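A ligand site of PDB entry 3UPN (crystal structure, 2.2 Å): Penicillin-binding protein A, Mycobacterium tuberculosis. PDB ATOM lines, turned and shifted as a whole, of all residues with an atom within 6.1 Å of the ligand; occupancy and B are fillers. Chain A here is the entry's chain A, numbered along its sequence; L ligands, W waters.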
ATOM      1  N   PRO A 191      21.672 -20.086  -7.340  1.00  0.00           N
ATOM      2  CA  PRO A 191      20.578 -21.060  -7.404  1.00  0.00           C
ATOM      3  C   PRO A 191      19.199 -20.487  -7.766  1.00  0.00           C
ATOM      4  O   PRO A 191      18.315 -21.252  -8.140  1.00  0.00           O
ATOM      5  CB  PRO A 191      20.566 -21.648  -5.983  1.00  0.00           C
ATOM      6  CG  PRO A 191      21.024 -20.536  -5.137  1.00  0.00           C
ATOM      7  CD  PRO A 191      22.101 -19.872  -5.950  1.00  0.00           C
ATOM      8  N   GLY A 192      19.018 -19.172  -7.638  1.00  0.00           N
ATOM      9  CA  GLY A 192      17.716 -18.527  -7.903  1.00  0.00           C
ATOM     10  C   GLY A 192      16.544 -19.201  -7.197  1.00  0.00           C
ATOM     11  O   GLY A 192      16.653 -19.573  -6.007  1.00  0.00           O
ATOM     12  N   SER A 193      15.443 -19.386  -7.927  1.00  0.00           N
ATOM     13  CA  SER A 193      14.209 -19.971  -7.376  1.00  0.00           C
ATOM     14  C   SER A 193      14.384 -21.294  -6.611  1.00  0.00           C
ATOM     15  O   SER A 193      13.620 -21.584  -5.682  1.00  0.00           O
ATOM     16  CB  SER A 193      13.133 -20.103  -8.477  1.00  0.00           C
ATOM     17  OG  SER A 193      12.408 -18.884  -8.706  1.00  0.00           O
ATOM     18  N   THR A 194      15.395 -22.094  -6.973  1.00  0.00           N
ATOM     19  CA  THR A 194      15.614 -23.379  -6.283  1.00  0.00           C
ATOM     20  C   THR A 194      15.953 -23.206  -4.795  1.00  0.00           C
ATOM     21  O   THR A 194      15.668 -24.087  -3.985  1.00  0.00           O
ATOM     22  CB  THR A 194      16.697 -24.258  -6.967  1.00  0.00           C
ATOM     23  OG1 THR A 194      17.967 -23.568  -6.952  1.00  0.00           O
ATOM     24  CG2 THR A 194      16.298 -24.597  -8.402  1.00  0.00           C
ATOM     25  N   LYS A 196      14.517 -21.397  -2.717  1.00  0.00           N
ATOM     26  CA  LYS A 196      13.322 -21.245  -1.906  1.00  0.00           C
ATOM     27  C   LYS A 196      13.114 -22.504  -1.083  1.00  0.00           C
ATOM     28  O   LYS A 196      12.498 -22.452  -0.026  1.00  0.00           O
ATOM     29  CB  LYS A 196      12.102 -20.906  -2.753  1.00  0.00           C
ATOM     30  CG  LYS A 196      12.147 -19.483  -3.318  1.00  0.00           C
ATOM     31  CD  LYS A 196      11.128 -19.250  -4.400  1.00  0.00           C
ATOM     32  CE  LYS A 196      11.241 -17.844  -4.932  1.00  0.00           C
ATOM     33  NZ  LYS A 196      10.150 -17.559  -5.885  1.00  0.00           N
ATOM     34  N   GLU A 230      10.675  -7.620  -7.239  1.00  0.00           N
ATOM     35  CA  GLU A 230       9.379  -7.802  -7.888  1.00  0.00           C
ATOM     36  C   GLU A 230       9.135  -9.265  -8.263  1.00  0.00           C
ATOM     37  O   GLU A 230      10.090 -10.013  -8.510  1.00  0.00           O
ATOM     38  CB  GLU A 230       9.272  -6.920  -9.149  1.00  0.00           C
ATOM     39  CG  GLU A 230      10.221  -7.327 -10.283  1.00  0.00           C
ATOM     40  CD  GLU A 230       9.923  -6.649 -11.624  1.00  0.00           C
ATOM     41  OE1 GLU A 230      10.222  -7.263 -12.678  1.00  0.00           O
ATOM     42  OE2 GLU A 230       9.408  -5.506 -11.620  1.00  0.00           O
ATOM     43  N   ASN A 231       7.871  -9.651  -8.342  1.00  0.00           N
ATOM     44  CA  ASN A 231       7.501 -10.926  -8.938  1.00  0.00           C
ATOM     45  C   ASN A 231       7.774 -10.936 -10.453  1.00  0.00           C
ATOM     46  O   ASN A 231       8.129  -9.913 -11.057  1.00  0.00           O
ATOM     47  CB  ASN A 231       6.025 -11.256  -8.700  1.00  0.00           C
ATOM     48  CG  ASN A 231       5.683 -11.511  -7.243  1.00  0.00           C
ATOM     49  OD1 ASN A 231       6.557 -11.647  -6.382  1.00  0.00           O
ATOM     50  ND2 ASN A 231       4.385 -11.583  -6.958  1.00  0.00           N
ATOM     51  N   TYR A 232       7.605 -12.107 -11.055  1.00  0.00           N
ATOM     52  CA  TYR A 232       7.684 -12.284 -12.490  1.00  0.00           C
ATOM     53  C   TYR A 232       6.316 -11.960 -13.109  1.00  0.00           C
ATOM     54  O   TYR A 232       5.314 -12.587 -12.745  1.00  0.00           O
ATOM     55  CB  TYR A 232       8.064 -13.746 -12.775  1.00  0.00           C
ATOM     56  CG  TYR A 232       8.661 -14.030 -14.125  1.00  0.00           C
ATOM     57  CD1 TYR A 232       9.447 -13.083 -14.792  1.00  0.00           C
ATOM     58  CD2 TYR A 232       8.486 -15.273 -14.728  1.00  0.00           C
ATOM     59  CE1 TYR A 232      10.007 -13.351 -16.033  1.00  0.00           C
ATOM     60  CE2 TYR A 232       9.046 -15.563 -15.967  1.00  0.00           C
ATOM     61  CZ  TYR A 232       9.809 -14.593 -16.618  1.00  0.00           C
ATOM     62  OH  TYR A 232      10.357 -14.873 -17.841  1.00  0.00           O
ATOM     63  N   VAL A 250       4.601 -23.137  -4.580  1.00  0.00           N
ATOM     64  CA  VAL A 250       4.347 -23.878  -5.818  1.00  0.00           C
ATOM     65  C   VAL A 250       4.264 -22.985  -7.066  1.00  0.00           C
ATOM     66  O   VAL A 250       4.511 -23.463  -8.177  1.00  0.00           O
ATOM     67  CB  VAL A 250       3.134 -24.856  -5.729  1.00  0.00           C
ATOM     68  CG1 VAL A 250       3.218 -25.714  -4.451  1.00  0.00           C
ATOM     69  CG2 VAL A 250       1.822 -24.124  -5.860  1.00  0.00           C
ATOM     70  N   LYS A 251       3.910 -21.721  -6.873  1.00  0.00           N
ATOM     71  CA  LYS A 251       3.808 -20.744  -7.967  1.00  0.00           C
ATOM     72  C   LYS A 251       5.064 -19.863  -8.014  1.00  0.00           C
ATOM     73  O   LYS A 251       5.175 -18.978  -8.857  1.00  0.00           O
ATOM     74  CB  LYS A 251       2.532 -19.906  -7.838  1.00  0.00           C
ATOM     75  CG  LYS A 251       1.229 -20.687  -8.050  1.00  0.00           C
ATOM     76  CD  LYS A 251       0.085 -19.794  -8.549  1.00  0.00           C
ATOM     77  CE  LYS A 251      -0.653 -19.099  -7.395  1.00  0.00           C
ATOM     78  NZ  LYS A 251      -2.020 -18.644  -7.811  1.00  0.00           N
ATOM     79  N   SER A 252       5.997 -20.138  -7.090  1.00  0.00           N
ATOM     80  CA  SER A 252       7.312 -19.489  -7.050  1.00  0.00           C
ATOM     81  C   SER A 252       7.245 -17.960  -7.052  1.00  0.00           C
ATOM     82  O   SER A 252       7.943 -17.303  -7.828  1.00  0.00           O
ATOM     83  CB  SER A 252       8.197 -19.990  -8.205  1.00  0.00           C
ATOM     84  OG  SER A 252       9.567 -19.974  -7.839  1.00  0.00           O
ATOM     85  N   ASN A 254       7.973 -14.252  -5.601  1.00  0.00           N
ATOM     86  CA  ASN A 254       9.214 -13.722  -5.042  1.00  0.00           C
ATOM     87  C   ASN A 254       9.034 -12.902  -3.791  1.00  0.00           C
ATOM     88  O   ASN A 254       9.750 -13.127  -2.815  1.00  0.00           O
ATOM     89  CB  ASN A 254       9.979 -12.902  -6.074  1.00  0.00           C
ATOM     90  CG  ASN A 254      10.827 -13.739  -7.000  1.00  0.00           C
ATOM     91  OD1 ASN A 254      10.972 -14.952  -6.812  1.00  0.00           O
ATOM     92  ND2 ASN A 254      11.402 -13.107  -8.007  1.00  0.00           N
ATOM     93  N   ILE A 308      15.569 -15.480  -2.168  1.00  0.00           N
ATOM     94  CA  ILE A 308      15.131 -15.911  -3.490  1.00  0.00           C
ATOM     95  C   ILE A 308      16.321 -16.339  -4.391  1.00  0.00           C
ATOM     96  O   ILE A 308      16.210 -16.354  -5.615  1.00  0.00           O
ATOM     97  CB  ILE A 308      14.210 -14.843  -4.174  1.00  0.00           C
ATOM     98  CG1 ILE A 308      15.010 -13.592  -4.577  1.00  0.00           C
ATOM     99  CG2 ILE A 308      13.009 -14.500  -3.264  1.00  0.00           C
ATOM    100  CD1 ILE A 308      14.321 -12.690  -5.591  1.00  0.00           C
ATOM    101  N   GLN A 310      19.540 -15.151  -4.802  1.00  0.00           N
ATOM    102  CA  GLN A 310      20.417 -14.198  -5.472  1.00  0.00           C
ATOM    103  C   GLN A 310      21.444 -13.633  -4.507  1.00  0.00           C
ATOM    104  O   GLN A 310      21.874 -14.328  -3.592  1.00  0.00           O
ATOM    105  CB  GLN A 310      19.606 -13.087  -6.156  1.00  0.00           C
ATOM    106  CG  GLN A 310      18.501 -13.589  -7.109  1.00  0.00           C
ATOM    107  CD  GLN A 310      19.008 -14.238  -8.396  1.00  0.00           C
ATOM    108  OE1 GLN A 310      18.212 -14.630  -9.247  1.00  0.00           O
ATOM    109  NE2 GLN A 310      20.338 -14.335  -8.554  1.00  0.00           N
ATOM    110  N   ALA A 381       4.296 -26.920 -12.763  1.00  0.00           N
ATOM    111  CA  ALA A 381       5.332 -26.778 -13.797  1.00  0.00           C
ATOM    112  C   ALA A 381       4.904 -27.258 -15.194  1.00  0.00           C
ATOM    113  O   ALA A 381       3.921 -27.996 -15.347  1.00  0.00           O
ATOM    114  CB  ALA A 381       6.622 -27.484 -13.357  1.00  0.00           C
ATOM    115  N   GLN A 382       5.633 -26.804 -16.222  1.00  0.00           N
ATOM    116  CA  GLN A 382       5.455 -27.309 -17.590  1.00  0.00           C
ATOM    117  C   GLN A 382       5.666 -28.822 -17.562  1.00  0.00           C
ATOM    118  O   GLN A 382       6.569 -29.305 -16.883  1.00  0.00           O
ATOM    119  CB  GLN A 382       6.455 -26.625 -18.524  1.00  0.00           C
ATOM    120  CG  GLN A 382       5.918 -26.312 -19.927  1.00  0.00           C
ATOM    121  CD  GLN A 382       6.366 -27.320 -20.993  1.00  0.00           C
ATOM    122  OE1 GLN A 382       7.518 -27.791 -20.990  1.00  0.00           O
ATOM    123  NE2 GLN A 382       5.456 -27.639 -21.920  1.00  0.00           N
ATOM    124  N   LYS A 395      11.694 -28.594  -7.877  1.00  0.00           N
ATOM    125  CA  LYS A 395      11.709 -27.140  -7.885  1.00  0.00           C
ATOM    126  C   LYS A 395      12.446 -26.643  -9.137  1.00  0.00           C
ATOM    127  O   LYS A 395      13.655 -26.875  -9.301  1.00  0.00           O
ATOM    128  CB  LYS A 395      12.344 -26.579  -6.623  1.00  0.00           C
ATOM    129  CG  LYS A 395      12.212 -25.071  -6.468  1.00  0.00           C
ATOM    130  CD  LYS A 395      10.769 -24.661  -6.145  1.00  0.00           C
ATOM    131  CE  LYS A 395      10.585 -23.153  -6.142  1.00  0.00           C
ATOM    132  NZ  LYS A 395      10.346 -22.631  -7.525  1.00  0.00           N
ATOM    133  N   THR A 396      11.702 -25.981 -10.028  1.00  0.00           N
ATOM    134  CA  THR A 396      12.261 -25.276 -11.181  1.00  0.00           C
ATOM    135  C   THR A 396      12.689 -23.879 -10.756  1.00  0.00           C
ATOM    136  O   THR A 396      12.316 -23.408  -9.682  1.00  0.00           O
ATOM    137  CB  THR A 396      11.215 -25.140 -12.315  1.00  0.00           C
ATOM    138  OG1 THR A 396      10.092 -24.402 -11.834  1.00  0.00           O
ATOM    139  CG2 THR A 396      10.727 -26.496 -12.796  1.00  0.00           C
ATOM    140  N   GLY A 397      13.454 -23.204 -11.594  1.00  0.00           N
ATOM    141  CA  GLY A 397      13.836 -21.833 -11.311  1.00  0.00           C
ATOM    142  C   GLY A 397      14.770 -21.187 -12.318  1.00  0.00           C
ATOM    143  O   GLY A 397      15.338 -21.862 -13.182  1.00  0.00           O
ATOM    144  N   THR A 398      14.928 -19.875 -12.182  1.00  0.00           N
ATOM    145  CA  THR A 398      15.896 -19.102 -12.962  1.00  0.00           C
ATOM    146  C   THR A 398      16.834 -18.392 -12.004  1.00  0.00           C
ATOM    147  O   THR A 398      16.542 -18.275 -10.809  1.00  0.00           O
ATOM    148  CB  THR A 398      15.210 -18.058 -13.909  1.00  0.00           C
ATOM    149  OG1 THR A 398      14.554 -17.047 -13.127  1.00  0.00           O
ATOM    150  CG2 THR A 398      14.213 -18.739 -14.830  1.00  0.00           C
ATOM    151  N   ALA A 399      17.969 -17.937 -12.521  1.00  0.00           N
ATOM    152  CA  ALA A 399      18.965 -17.228 -11.711  1.00  0.00           C
ATOM    153  C   ALA A 399      19.710 -16.197 -12.539  1.00  0.00           C
ATOM    154  O   ALA A 399      20.253 -16.517 -13.597  1.00  0.00           O
ATOM    155  CB  ALA A 399      19.926 -18.216 -11.092  1.00  0.00           C
ATOM    156  N   ASP A 436      13.888 -18.755 -20.337  1.00  0.00           N
ATOM    157  CA  ASP A 436      13.075 -18.044 -21.342  1.00  0.00           C
ATOM    158  C   ASP A 436      12.316 -16.882 -20.706  1.00  0.00           C
ATOM    159  O   ASP A 436      12.662 -16.446 -19.597  1.00  0.00           O
ATOM    160  CB  ASP A 436      12.151 -19.024 -22.094  1.00  0.00           C
ATOM    161  CG  ASP A 436      11.167 -19.728 -21.185  1.00  0.00           C
ATOM    162  OD1 ASP A 436       9.950 -19.472 -21.322  1.00  0.00           O
ATOM    163  OD2 ASP A 436      11.598 -20.528 -20.322  1.00  0.00           O
ATOM    164  N   ALA A 444      10.971 -24.702 -18.405  1.00  0.00           N
ATOM    165  CA  ALA A 444      10.728 -24.893 -19.843  1.00  0.00           C
ATOM    166  C   ALA A 444      11.870 -25.624 -20.546  1.00  0.00           C
ATOM    167  O   ALA A 444      11.623 -26.544 -21.334  1.00  0.00           O
ATOM    168  CB  ALA A 444      10.438 -23.569 -20.524  1.00  0.00           C
ATOM    169  N   ALA A 447      13.640 -28.448 -17.115  1.00  0.00           N
ATOM    170  CA  ALA A 447      12.791 -29.531 -16.601  1.00  0.00           C
ATOM    171  C   ALA A 447      12.684 -30.805 -17.459  1.00  0.00           C
ATOM    172  O   ALA A 447      12.826 -31.902 -16.919  1.00  0.00           O
ATOM    173  CB  ALA A 447      11.391 -29.012 -16.206  1.00  0.00           C
ATOM    174  N   ARG A 451      13.770 -34.664 -16.376  1.00  0.00           N
ATOM    175  CA  ARG A 451      12.822 -35.772 -16.461  1.00  0.00           C
ATOM    176  C   ARG A 451      13.273 -36.937 -17.328  1.00  0.00           C
ATOM    177  O   ARG A 451      12.898 -38.075 -17.057  1.00  0.00           O
ATOM    178  CB  ARG A 451      11.448 -35.276 -16.949  1.00  0.00           C
ATOM    179  CG  ARG A 451      10.733 -34.359 -15.983  1.00  0.00           C
ATOM    180  CD  ARG A 451       9.369 -33.914 -16.532  1.00  0.00           C
ATOM    181  NE  ARG A 451       8.774 -32.929 -15.633  1.00  0.00           N
ATOM    182  CZ  ARG A 451       8.454 -31.681 -15.978  1.00  0.00           C
ATOM    183  NH1 ARG A 451       8.612 -31.266 -17.217  1.00  0.00           N
ATOM    184  NH2 ARG A 451       7.956 -30.864 -15.076  1.00  0.00           N
HETATM  185  C1  LIG L   1      12.936 -17.883  -9.507  1.00  0.00           C
HETATM  186  C2  LIG L   1      10.301 -18.925 -12.704  1.00  0.00           C
HETATM  187  C3  LIG L   1      12.205 -17.191 -10.659  1.00  0.00           C
HETATM  188  C4  LIG L   1      10.702 -17.503 -10.850  1.00  0.00           C
HETATM  189  C5  LIG L   1      10.106 -19.629 -11.591  1.00  0.00           C
HETATM  190  O1  LIG L   1      14.085 -17.536  -9.267  1.00  0.00           O
HETATM  191  C6  LIG L   1      12.516 -15.665 -10.699  1.00  0.00           C
HETATM  192  O2  LIG L   1      13.397 -15.252  -9.645  1.00  0.00           O
HETATM  193  C7  LIG L   1      11.295 -14.758 -10.695  1.00  0.00           C
HETATM  194  N1  LIG L   1      10.458 -18.911 -10.544  1.00  0.00           N
HETATM  195  C8  LIG L   1       9.588 -20.992 -11.451  1.00  0.00           C
HETATM  196  O3  LIG L   1       8.347 -21.173 -11.351  1.00  0.00           O
HETATM  197  O4  LIG L   1      10.406 -21.936 -11.443  1.00  0.00           O
HETATM  198  S1  LIG L   1      10.541 -19.516 -14.256  1.00  0.00           S
HETATM  199  C9  LIG L   1       9.184 -20.504 -14.818  1.00  0.00           C
HETATM  200  C10 LIG L   1       9.664 -21.916 -15.161  1.00  0.00           C
HETATM  201  N2  LIG L   1       8.469 -22.757 -15.214  1.00  0.00           N
HETATM  202  C11 LIG L   1       8.564 -23.974 -15.251  1.00  0.00           C
HETATM  203  N3  LIG L   1       8.775 -25.155 -15.478  1.00  0.00           N
HETATM  204  C12 LIG L   1      10.345 -17.465 -12.344  1.00  0.00           C
HETATM  205  O   HOH W   1       6.064 -22.571 -10.963  1.00  0.00           O
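The backbone NH (N) of Ser 193 is in hydrogen-bond range of an oxygen (O1) of the ligand, 2.7 Å away. OG of Ser 193 is covalently linked to C1 of the ligand (1.4 Å). O4 of the ligand lies close to O of Thr 396, 3.0 Å away. O4 of the ligand lies within hydrogen-bond range of OG1 of Thr 396 (2.5 Å). A nitrogen (N1) of the ligand lies within hydrogen-bond range of the side-chain hydroxyl of Ser 252 (3.0 Å). ND2 of Asn 254 lies close to O2 of the ligand, at 3.4 Å. The backbone NH (N) of Gly 397 lies within hydrogen-bond range of an oxygen (O4) of the ligand, at 3.3 Å. The side-chain amino group (NZ) of Lys 395 lies within salt-bridge range of an oxygen (O4) of the ligand, at 3.98 Å.
The backbone NH of Ser 193 lies within hydrogen-bond range of the backbone carbonyl oxygen of Thr 398, at 3.3 Å. The side-chain hydroxyl of Ser 193 sits at hydrogen-bond distance from the side-chain hydroxyl of Ser 252 (3.2 Å). The side-chain hydroxyl (OG) of Ser 252 is in hydrogen-bond range of the side-chain amino group (NZ) of Lys 395 (2.8 Å). O of Ser 252 lies within hydrogen-bond range of NZ of Lys 196 (3.0 Å). N of Asn 254 sits at hydrogen-bond distance from OD1 of Asn 231 (3.1 Å). ND2 of Asn 254 sits at hydrogen-bond distance from O of Glu 230 (3.4 Å). The backbone carbonyl oxygen (O) of Gln 382 sits at hydrogen-bond distance from the guanidinium group (NH2) of Arg 451 (2.8 Å). The side-chain hydroxyl (OH) of Tyr 232 is in hydrogen-bond range of the backbone carbonyl oxygen (O) of Asp 436, at 3.3 Å.
An oxygen (O1) of the ligand sits close to the backbone carbonyl oxygen (O) of Thr 398 (3.0 Å). Gly 192 touches the ligand (C to O1, 3.6 Å). CD2 of Tyr 232 touches C12 of the ligand (3.7 Å). Ala 381 touches the ligand. N of Gln 382 touches N3 of the ligand (3.6 Å). Ala 444 touches the ligand (N to N3, 3.7 Å). Hydrophobic or aromatic side chains that line the ligand: Tyr 232 and Ala 381.
Water W1 lies within hydrogen-bond range of an oxygen (O3) of the ligand and the backbone carbonyl oxygen of Val 250.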
